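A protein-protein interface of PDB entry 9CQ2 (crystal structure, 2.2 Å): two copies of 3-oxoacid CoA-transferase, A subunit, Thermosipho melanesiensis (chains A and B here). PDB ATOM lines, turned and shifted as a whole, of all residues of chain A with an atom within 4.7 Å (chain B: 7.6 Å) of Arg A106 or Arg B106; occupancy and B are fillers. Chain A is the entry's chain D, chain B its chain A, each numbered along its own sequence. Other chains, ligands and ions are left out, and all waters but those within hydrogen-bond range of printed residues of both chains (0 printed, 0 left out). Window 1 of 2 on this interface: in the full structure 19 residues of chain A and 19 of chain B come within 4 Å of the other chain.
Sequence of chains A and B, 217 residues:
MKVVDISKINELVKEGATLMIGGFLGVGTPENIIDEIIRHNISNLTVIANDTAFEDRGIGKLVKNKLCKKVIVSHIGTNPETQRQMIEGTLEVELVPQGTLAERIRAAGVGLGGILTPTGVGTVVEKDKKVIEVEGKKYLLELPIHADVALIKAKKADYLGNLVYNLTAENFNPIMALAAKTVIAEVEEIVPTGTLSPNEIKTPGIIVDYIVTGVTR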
ATOM      1  N   ALA A 102     -28.015  13.224  11.604  1.00  0.00           N
ATOM      2  CA  ALA A 102     -27.528  12.518  10.422  1.00  0.00           C
ATOM      3  C   ALA A 102     -26.214  11.802  10.721  1.00  0.00           C
ATOM      4  O   ALA A 102     -26.033  10.632  10.361  1.00  0.00           O
ATOM      5  CB  ALA A 102     -27.351  13.483   9.235  1.00  0.00           C
ATOM      6  N   GLU A 103     -25.266  12.496  11.371  1.00  0.00           N
ATOM      7  CA  GLU A 103     -23.938  11.908  11.568  1.00  0.00           C
ATOM      8  C   GLU A 103     -23.898  10.867  12.685  1.00  0.00           C
ATOM      9  O   GLU A 103     -23.057   9.960  12.652  1.00  0.00           O
ATOM     10  CB  GLU A 103     -22.910  12.991  11.882  1.00  0.00           C
ATOM     11  CG  GLU A 103     -22.651  13.968  10.730  1.00  0.00           C
ATOM     12  CD  GLU A 103     -21.936  13.318   9.553  1.00  0.00           C
ATOM     13  OE1 GLU A 103     -20.957  12.582   9.815  1.00  0.00           O
ATOM     14  OE2 GLU A 103     -22.334  13.565   8.380  1.00  0.00           O
ATOM     15  N   ARG A 104     -24.758  11.001  13.691  1.00  0.00           N
ATOM     16  CA  ARG A 104     -24.846   9.966  14.714  1.00  0.00           C
ATOM     17  C   ARG A 104     -25.400   8.667  14.140  1.00  0.00           C
ATOM     18  O   ARG A 104     -24.888   7.590  14.458  1.00  0.00           O
ATOM     19  CB  ARG A 104     -25.724  10.451  15.878  1.00  0.00           C
ATOM     20  CG  ARG A 104     -25.050  11.529  16.730  1.00  0.00           C
ATOM     21  CD  ARG A 104     -25.907  12.005  17.868  1.00  0.00           C
ATOM     22  NE  ARG A 104     -26.129  10.948  18.840  1.00  0.00           N
ATOM     23  CZ  ARG A 104     -27.114  10.942  19.730  1.00  0.00           C
ATOM     24  NH1 ARG A 104     -27.940  11.973  19.859  1.00  0.00           N
ATOM     25  NH2 ARG A 104     -27.280   9.866  20.500  1.00  0.00           N
ATOM     26  N   ILE A 105     -26.460   8.751  13.320  1.00  0.00           N
ATOM     27  CA  ILE A 105     -26.973   7.561  12.648  1.00  0.00           C
ATOM     28  C   ILE A 105     -25.919   6.999  11.702  1.00  0.00           C
ATOM     29  O   ILE A 105     -25.585   5.802  11.730  1.00  0.00           O
ATOM     30  CB  ILE A 105     -28.277   7.900  11.907  1.00  0.00           C
ATOM     31  CG1 ILE A 105     -29.367   8.327  12.893  1.00  0.00           C
ATOM     32  CG2 ILE A 105     -28.702   6.721  11.030  1.00  0.00           C
ATOM     33  CD1 ILE A 105     -30.672   8.793  12.269  1.00  0.00           C
ATOM     34  N   ARG A 106     -25.365   7.862  10.853  1.00  0.00           N
ATOM     35  CA  ARG A 106     -24.331   7.400   9.948  1.00  0.00           C
ATOM     36  C   ARG A 106     -23.208   6.731  10.713  1.00  0.00           C
ATOM     37  O   ARG A 106     -22.623   5.752  10.238  1.00  0.00           O
ATOM     38  CB  ARG A 106     -23.756   8.567   9.145  1.00  0.00           C
ATOM     39  CG  ARG A 106     -22.560   8.194   8.293  1.00  0.00           C
ATOM     40  CD  ARG A 106     -22.013   9.365   7.424  1.00  0.00           C
ATOM     41  NE  ARG A 106     -21.007   8.869   6.495  1.00  0.00           N
ATOM     42  CZ  ARG A 106     -19.755   8.623   6.823  1.00  0.00           C
ATOM     43  NH1 ARG A 106     -19.308   8.828   8.059  1.00  0.00           N
ATOM     44  NH2 ARG A 106     -18.927   8.165   5.894  1.00  0.00           N
ATOM     45  N   ALA A 107     -22.829   7.286  11.867  1.00  0.00           N
ATOM     46  CA  ALA A 107     -21.696   6.698  12.576  1.00  0.00           C
ATOM     47  C   ALA A 107     -21.968   5.226  12.925  1.00  0.00           C
ATOM     48  O   ALA A 107     -21.085   4.374  12.775  1.00  0.00           O
ATOM     49  CB  ALA A 107     -21.392   7.509  13.827  1.00  0.00           C
ATOM     50  N   ALA A 108     -23.187   4.913  13.389  1.00  0.00           N
ATOM     51  CA  ALA A 108     -23.562   3.517  13.644  1.00  0.00           C
ATOM     52  C   ALA A 108     -23.487   2.699  12.362  1.00  0.00           C
ATOM     53  O   ALA A 108     -22.980   1.569  12.354  1.00  0.00           O
ATOM     54  CB  ALA A 108     -24.965   3.463  14.242  1.00  0.00           C
ATOM     55  N   GLY A 109     -23.927   3.293  11.250  1.00  0.00           N
ATOM     56  CA  GLY A 109     -23.927   2.589   9.986  1.00  0.00           C
ATOM     57  C   GLY A 109     -22.560   2.245   9.454  1.00  0.00           C
ATOM     58  O   GLY A 109     -22.409   1.237   8.760  1.00  0.00           O
ATOM     59  N   VAL A 110     -21.561   3.090   9.697  1.00  0.00           N
ATOM     60  CA  VAL A 110     -20.230   2.874   9.116  1.00  0.00           C
ATOM     61  C   VAL A 110     -19.252   2.405  10.166  1.00  0.00           C
ATOM     62  O   VAL A 110     -18.060   2.267   9.887  1.00  0.00           O
ATOM     63  CB  VAL A 110     -19.704   4.125   8.388  1.00  0.00           C
ATOM     64  CG1 VAL A 110     -20.694   4.543   7.268  1.00  0.00           C
ATOM     65  CG2 VAL A 110     -19.430   5.325   9.344  1.00  0.00           C
ATOM     66  N   LEU A 112     -18.389   3.740  13.280  1.00  0.00           N
ATOM     67  CA  LEU A 112     -17.587   4.648  14.076  1.00  0.00           C
ATOM     68  C   LEU A 112     -18.082   4.657  15.511  1.00  0.00           C
ATOM     69  O   LEU A 112     -19.263   4.387  15.784  1.00  0.00           O
ATOM     70  CB  LEU A 112     -17.622   6.068  13.505  1.00  0.00           C
ATOM     71  CG  LEU A 112     -17.013   6.248  12.103  1.00  0.00           C
ATOM     72  CD1 LEU A 112     -17.365   7.675  11.605  1.00  0.00           C
ATOM     73  CD2 LEU A 112     -15.526   6.022  12.007  1.00  0.00           C
ATOM     74  N   ILE A 175     -29.189   6.594   4.986  1.00  0.00           N
ATOM     75  CA  ILE A 175     -28.329   6.570   6.163  1.00  0.00           C
ATOM     76  C   ILE A 175     -28.844   5.537   7.150  1.00  0.00           C
ATOM     77  O   ILE A 175     -28.078   4.757   7.724  1.00  0.00           O
ATOM     78  CB  ILE A 175     -28.293   7.955   6.829  1.00  0.00           C
ATOM     79  CG1 ILE A 175     -28.183   9.112   5.838  1.00  0.00           C
ATOM     80  CG2 ILE A 175     -27.154   8.014   7.847  1.00  0.00           C
ATOM     81  CD1 ILE A 175     -28.347  10.449   6.541  1.00  0.00           C
ATOM     82  N   MET B  20      -4.674  17.312  -1.958  1.00  0.00           N
ATOM     83  CA  MET B  20      -5.340  16.018  -2.077  1.00  0.00           C
ATOM     84  C   MET B  20      -5.438  15.672  -3.562  1.00  0.00           C
ATOM     85  O   MET B  20      -5.816  16.527  -4.382  1.00  0.00           O
ATOM     86  CB  MET B  20      -6.735  15.920  -1.441  1.00  0.00           C
ATOM     87  CG  MET B  20      -6.742  16.213   0.066  1.00  0.00           C
ATOM     88  SD  MET B  20      -8.283  16.898   0.587  1.00  0.00           S
ATOM     89  CE  MET B  20      -8.024  16.801   2.406  1.00  0.00           C
ATOM     90  N   THR B 100      -9.666   4.937   7.605  1.00  0.00           N
ATOM     91  CA  THR B 100      -9.426   6.105   8.457  1.00  0.00           C
ATOM     92  C   THR B 100      -9.097   7.335   7.620  1.00  0.00           C
ATOM     93  O   THR B 100      -9.609   8.435   7.877  1.00  0.00           O
ATOM     94  CB  THR B 100      -8.290   5.765   9.421  1.00  0.00           C
ATOM     95  OG1 THR B 100      -8.743   4.699  10.281  1.00  0.00           O
ATOM     96  CG2 THR B 100      -7.847   6.961  10.268  1.00  0.00           C
ATOM     97  N   LEU B 101      -8.299   7.136   6.575  1.00  0.00           N
ATOM     98  CA  LEU B 101      -8.014   8.207   5.622  1.00  0.00           C
ATOM     99  C   LEU B 101      -9.295   8.725   4.987  1.00  0.00           C
ATOM    100  O   LEU B 101      -9.546   9.930   4.977  1.00  0.00           O
ATOM    101  CB  LEU B 101      -7.065   7.705   4.560  1.00  0.00           C
ATOM    102  CG  LEU B 101      -6.470   8.736   3.612  1.00  0.00           C
ATOM    103  CD1 LEU B 101      -5.501   9.599   4.363  1.00  0.00           C
ATOM    104  CD2 LEU B 101      -5.798   7.978   2.493  1.00  0.00           C
ATOM    105  N   ALA B 102     -10.145   7.817   4.491  1.00  0.00           N
ATOM    106  CA  ALA B 102     -11.426   8.240   3.948  1.00  0.00           C
ATOM    107  C   ALA B 102     -12.202   9.081   4.954  1.00  0.00           C
ATOM    108  O   ALA B 102     -12.727  10.141   4.601  1.00  0.00           O
ATOM    109  CB  ALA B 102     -12.231   7.006   3.503  1.00  0.00           C
ATOM    110  N   GLU B 103     -12.270   8.648   6.229  1.00  0.00           N
ATOM    111  CA  GLU B 103     -13.097   9.389   7.179  1.00  0.00           C
ATOM    112  C   GLU B 103     -12.443  10.677   7.681  1.00  0.00           C
ATOM    113  O   GLU B 103     -13.157  11.605   8.082  1.00  0.00           O
ATOM    114  CB  GLU B 103     -13.476   8.501   8.370  1.00  0.00           C
ATOM    115  CG  GLU B 103     -14.475   7.374   7.992  1.00  0.00           C
ATOM    116  CD  GLU B 103     -15.856   7.863   7.557  1.00  0.00           C
ATOM    117  OE1 GLU B 103     -16.459   8.733   8.248  1.00  0.00           O
ATOM    118  OE2 GLU B 103     -16.358   7.339   6.530  1.00  0.00           O
ATOM    119  N   ARG B 104     -11.107  10.735   7.720  1.00  0.00           N
ATOM    120  CA  ARG B 104     -10.419  11.958   8.127  1.00  0.00           C
ATOM    121  C   ARG B 104     -10.563  13.042   7.062  1.00  0.00           C
ATOM    122  O   ARG B 104     -10.822  14.212   7.374  1.00  0.00           O
ATOM    123  CB  ARG B 104      -8.943  11.645   8.387  1.00  0.00           C
ATOM    124  CG  ARG B 104      -8.737  10.732   9.627  1.00  0.00           C
ATOM    125  CD  ARG B 104      -7.258  10.438   9.881  1.00  0.00           C
ATOM    126  NE  ARG B 104      -6.495  11.654  10.154  1.00  0.00           N
ATOM    127  CZ  ARG B 104      -5.173  11.751  10.060  1.00  0.00           C
ATOM    128  NH1 ARG B 104      -4.416  10.706   9.721  1.00  0.00           N
ATOM    129  NH2 ARG B 104      -4.594  12.924  10.307  1.00  0.00           N
ATOM    130  N   ILE B 105     -10.390  12.669   5.797  1.00  0.00           N
ATOM    131  CA  ILE B 105     -10.668  13.612   4.716  1.00  0.00           C
ATOM    132  C   ILE B 105     -12.111  14.042   4.795  1.00  0.00           C
ATOM    133  O   ILE B 105     -12.425  15.244   4.767  1.00  0.00           O
ATOM    134  CB  ILE B 105     -10.327  12.984   3.358  1.00  0.00           C
ATOM    135  CG1 ILE B 105      -8.829  12.693   3.302  1.00  0.00           C
ATOM    136  CG2 ILE B 105     -10.752  13.890   2.201  1.00  0.00           C
ATOM    137  CD1 ILE B 105      -8.384  11.911   2.064  1.00  0.00           C
ATOM    138  N   ARG B 106     -13.021  13.078   4.978  1.00  0.00           N
ATOM    139  CA  ARG B 106     -14.425  13.441   4.999  1.00  0.00           C
ATOM    140  C   ARG B 106     -14.733  14.397   6.150  1.00  0.00           C
ATOM    141  O   ARG B 106     -15.473  15.378   5.973  1.00  0.00           O
ATOM    142  CB  ARG B 106     -15.301  12.186   5.088  1.00  0.00           C
ATOM    143  CG  ARG B 106     -16.792  12.499   5.067  1.00  0.00           C
ATOM    144  CD  ARG B 106     -17.694  11.240   5.316  1.00  0.00           C
ATOM    145  NE  ARG B 106     -19.102  11.599   5.375  1.00  0.00           N
ATOM    146  CZ  ARG B 106     -19.736  12.032   6.459  1.00  0.00           C
ATOM    147  NH1 ARG B 106     -19.131  12.113   7.627  1.00  0.00           N
ATOM    148  NH2 ARG B 106     -21.019  12.400   6.363  1.00  0.00           N
ATOM    149  N   ALA B 107     -14.182  14.121   7.338  1.00  0.00           N
ATOM    150  CA  ALA B 107     -14.395  14.991   8.489  1.00  0.00           C
ATOM    151  C   ALA B 107     -14.108  16.456   8.141  1.00  0.00           C
ATOM    152  O   ALA B 107     -14.899  17.350   8.467  1.00  0.00           O
ATOM    153  CB  ALA B 107     -13.500  14.514   9.644  1.00  0.00           C
ATOM    154  N   ALA B 108     -12.975  16.711   7.483  1.00  0.00           N
ATOM    155  CA  ALA B 108     -12.676  18.062   7.011  1.00  0.00           C
ATOM    156  C   ALA B 108     -13.736  18.552   6.039  1.00  0.00           C
ATOM    157  O   ALA B 108     -14.184  19.692   6.126  1.00  0.00           O
ATOM    158  CB  ALA B 108     -11.309  18.084   6.346  1.00  0.00           C
ATOM    159  N   GLY B 109     -14.176  17.689   5.124  1.00  0.00           N
ATOM    160  CA  GLY B 109     -15.140  18.109   4.138  1.00  0.00           C
ATOM    161  C   GLY B 109     -16.482  18.513   4.705  1.00  0.00           C
ATOM    162  O   GLY B 109     -17.130  19.415   4.165  1.00  0.00           O
ATOM    163  N   VAL B 110     -16.932  17.852   5.778  1.00  0.00           N
ATOM    164  CA  VAL B 110     -18.283  18.049   6.307  1.00  0.00           C
ATOM    165  C   VAL B 110     -18.282  18.804   7.631  1.00  0.00           C
ATOM    166  O   VAL B 110     -19.336  18.923   8.275  1.00  0.00           O
ATOM    167  CB  VAL B 110     -19.019  16.705   6.450  1.00  0.00           C
ATOM    168  CG1 VAL B 110     -19.068  16.014   5.075  1.00  0.00           C
ATOM    169  CG2 VAL B 110     -18.326  15.776   7.478  1.00  0.00           C
ATOM    170  N   GLY B 111     -17.130  19.285   8.076  1.00  0.00           N
ATOM    171  CA  GLY B 111     -17.120  20.198   9.209  1.00  0.00           C
ATOM    172  C   GLY B 111     -17.078  19.524  10.560  1.00  0.00           C
ATOM    173  O   GLY B 111     -17.565  20.086  11.542  1.00  0.00           O
ATOM    174  N   LEU B 112     -16.538  18.321  10.627  1.00  0.00           N
ATOM    175  CA  LEU B 112     -16.406  17.603  11.884  1.00  0.00           C
ATOM    176  C   LEU B 112     -15.027  17.844  12.469  1.00  0.00           C
ATOM    177  O   LEU B 112     -14.047  18.025  11.736  1.00  0.00           O
ATOM    178  CB  LEU B 112     -16.590  16.097  11.687  1.00  0.00           C
ATOM    179  CG  LEU B 112     -17.970  15.599  11.241  1.00  0.00           C
ATOM    180  CD1 LEU B 112     -17.895  14.104  10.957  1.00  0.00           C
ATOM    181  CD2 LEU B 112     -19.056  15.898  12.272  1.00  0.00           C
ATOM    182  N   ILE B 115     -13.223  11.954  14.219  1.00  0.00           N
ATOM    183  CA  ILE B 115     -14.053  10.757  14.234  1.00  0.00           C
ATOM    184  C   ILE B 115     -13.343   9.700  15.060  1.00  0.00           C
ATOM    185  O   ILE B 115     -12.105   9.644  15.084  1.00  0.00           O
ATOM    186  CB  ILE B 115     -14.355  10.217  12.821  1.00  0.00           C
ATOM    187  CG1 ILE B 115     -13.101  10.122  11.938  1.00  0.00           C
ATOM    188  CG2 ILE B 115     -15.266  11.159  12.066  1.00  0.00           C
ATOM    189  CD1 ILE B 115     -12.529   8.779  11.881  1.00  0.00           C
ATOM    190  N   PRO B 144      -9.349  15.554  11.447  1.00  0.00           N
ATOM    191  CA  PRO B 144      -9.611  16.021  10.078  1.00  0.00           C
ATOM    192  C   PRO B 144      -8.315  16.332   9.347  1.00  0.00           C
ATOM    193  O   PRO B 144      -7.379  16.892   9.921  1.00  0.00           O
ATOM    194  CB  PRO B 144     -10.462  17.279  10.290  1.00  0.00           C
ATOM    195  CG  PRO B 144     -11.030  17.131  11.724  1.00  0.00           C
ATOM    196  CD  PRO B 144      -9.988  16.397  12.483  1.00  0.00           C
ATOM    197  N   ILE B 145      -8.254  15.926   8.076  1.00  0.00           N
ATOM    198  CA  ILE B 145      -7.151  16.259   7.167  1.00  0.00           C
ATOM    199  C   ILE B 145      -7.608  17.350   6.195  1.00  0.00           C
ATOM    200  O   ILE B 145      -8.612  17.190   5.482  1.00  0.00           O
ATOM    201  CB  ILE B 145      -6.674  15.025   6.385  1.00  0.00           C
ATOM    202  CG1 ILE B 145      -6.123  13.997   7.356  1.00  0.00           C
ATOM    203  CG2 ILE B 145      -5.596  15.400   5.373  1.00  0.00           C
ATOM    204  CD1 ILE B 145      -5.814  12.613   6.741  1.00  0.00           C
ATOM    205  N   PHE B 172     -11.620   8.158  -3.910  1.00  0.00           N
ATOM    206  CA  PHE B 172     -11.501   9.310  -2.994  1.00  0.00           C
ATOM    207  C   PHE B 172     -11.932  10.657  -3.593  1.00  0.00           C
ATOM    208  O   PHE B 172     -12.052  11.644  -2.842  1.00  0.00           O
ATOM    209  CB  PHE B 172     -10.039   9.449  -2.472  1.00  0.00           C
ATOM    210  CG  PHE B 172      -9.702   8.468  -1.374  1.00  0.00           C
ATOM    211  CD1 PHE B 172      -9.256   7.182  -1.692  1.00  0.00           C
ATOM    212  CD2 PHE B 172      -9.832   8.822  -0.046  1.00  0.00           C
ATOM    213  CE1 PHE B 172      -8.980   6.262  -0.688  1.00  0.00           C
ATOM    214  CE2 PHE B 172      -9.553   7.906   0.962  1.00  0.00           C
ATOM    215  CZ  PHE B 172      -9.138   6.628   0.644  1.00  0.00           C
ATOM    216  N   ILE B 175     -14.773  12.803  -2.100  1.00  0.00           N
ATOM    217  CA  ILE B 175     -14.502  13.148  -0.709  1.00  0.00           C
ATOM    218  C   ILE B 175     -13.543  14.330  -0.618  1.00  0.00           C
ATOM    219  O   ILE B 175     -13.728  15.264   0.167  1.00  0.00           O
ATOM    220  CB  ILE B 175     -13.897  11.936   0.003  1.00  0.00           C
ATOM    221  CG1 ILE B 175     -14.725  10.678  -0.236  1.00  0.00           C
ATOM    222  CG2 ILE B 175     -13.812  12.190   1.454  1.00  0.00           C
ATOM    223  CD1 ILE B 175     -14.004   9.440   0.262  1.00  0.00           C
ATOM    224  N   MET B 176     -12.462  14.233  -1.358  1.00  0.00           N
ATOM    225  CA  MET B 176     -11.504  15.306  -1.499  1.00  0.00           C
ATOM    226  C   MET B 176     -12.154  16.592  -2.014  1.00  0.00           C
ATOM    227  O   MET B 176     -11.834  17.686  -1.548  1.00  0.00           O
ATOM    228  CB  MET B 176     -10.450  14.772  -2.448  1.00  0.00           C
ATOM    229  CG  MET B 176      -9.567  13.685  -1.821  1.00  0.00           C
ATOM    230  SD  MET B 176      -8.362  13.055  -2.918  1.00  0.00           S
ATOM    231  CE  MET B 176      -7.428  11.990  -1.864  1.00  0.00           C
ATOM    232  N   LEU B 178     -14.783  17.853  -1.196  1.00  0.00           N
ATOM    233  CA  LEU B 178     -15.414  18.613  -0.130  1.00  0.00           C
ATOM    234  C   LEU B 178     -14.406  19.148   0.866  1.00  0.00           C
ATOM    235  O   LEU B 178     -14.738  20.044   1.654  1.00  0.00           O
ATOM    236  CB  LEU B 178     -16.408  17.715   0.617  1.00  0.00           C
ATOM    237  CG  LEU B 178     -17.697  17.300  -0.076  1.00  0.00           C
ATOM    238  CD1 LEU B 178     -18.142  15.963   0.528  1.00  0.00           C
ATOM    239  CD2 LEU B 178     -18.763  18.373   0.124  1.00  0.00           C
ATOM    240  N   ALA B 179     -13.202  18.593   0.869  1.00  0.00           N
ATOM    241  CA  ALA B 179     -12.284  18.813   1.971  1.00  0.00           C
ATOM    242  C   ALA B 179     -11.305  19.954   1.728  1.00  0.00           C
ATOM    243  O   ALA B 179     -10.929  20.630   2.675  1.00  0.00           O
ATOM    244  CB  ALA B 179     -11.493  17.528   2.274  1.00  0.00           C
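OE2 of Glu B103 lies within salt-bridge range of NH2 of Arg A106, at 2.8 Å. OE2 of Glu A103 is in salt-bridge range of NH2 of Arg B106, at 2.7 Å. The guanidinium group of Arg B106 sits close to the guanidinium group of Arg A106, 3.3 Å away.
Printed residues of chain A that touch a printed residue of chain B: Glu A103, Arg A106 and Leu A112. Of the 22 printed residues of chain B, 3 touch a printed residue of chain A. Printed residues of chain B that touch a printed residue of chain A: Glu B103, Arg B106 and Leu B112.
Among the printed residues, merely in contact across the chains: Glu A103 with Leu B112 (3.6 Å) and Leu A112 with Glu B103 (3.6 Å).
O of Ala B107 sits at hydrogen-bond distance from N of Leu B112 (2.9 Å). The backbone carbonyl oxygen (O) of Ala A107 lies within hydrogen-bond range of the backbone NH (N) of Leu A112, 2.8 Å away.
Printed residues of chain B within 4 Å of Glu A103: Arg B106 (2.7 Å) and Leu B112 (3.6 Å). Arg A106 touches two residues of chain B. Printed residues of chain B within 4 Å of Leu A112: Glu B103 (3.6 Å). Of the printed residues of chain A, Glu B103 touches Arg A106 (2.8 Å) and Leu A112 (3.6 Å). Of the printed residues of chain A, Arg B106 touches Glu A103 and Arg A106. Of the printed residues of chain A, Leu B112 touches Glu A103. The nearest residue of chain B that does not touch Arg A106 is Ile B115 (6.2 Å).
Glu A103 touches Arg B106, and with the chains exchanged Arg A106 touches Glu B103. Glu A103 touches Leu B112, and with the chains exchanged Leu A112 touches Glu B103. Arg B106 touches its own counterpart, Arg A106. 11 positions are printed for both chains. Of the 5 pairs that touch across the chains among the printed residues, 5 have their exchanged pair printed and touching as well.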
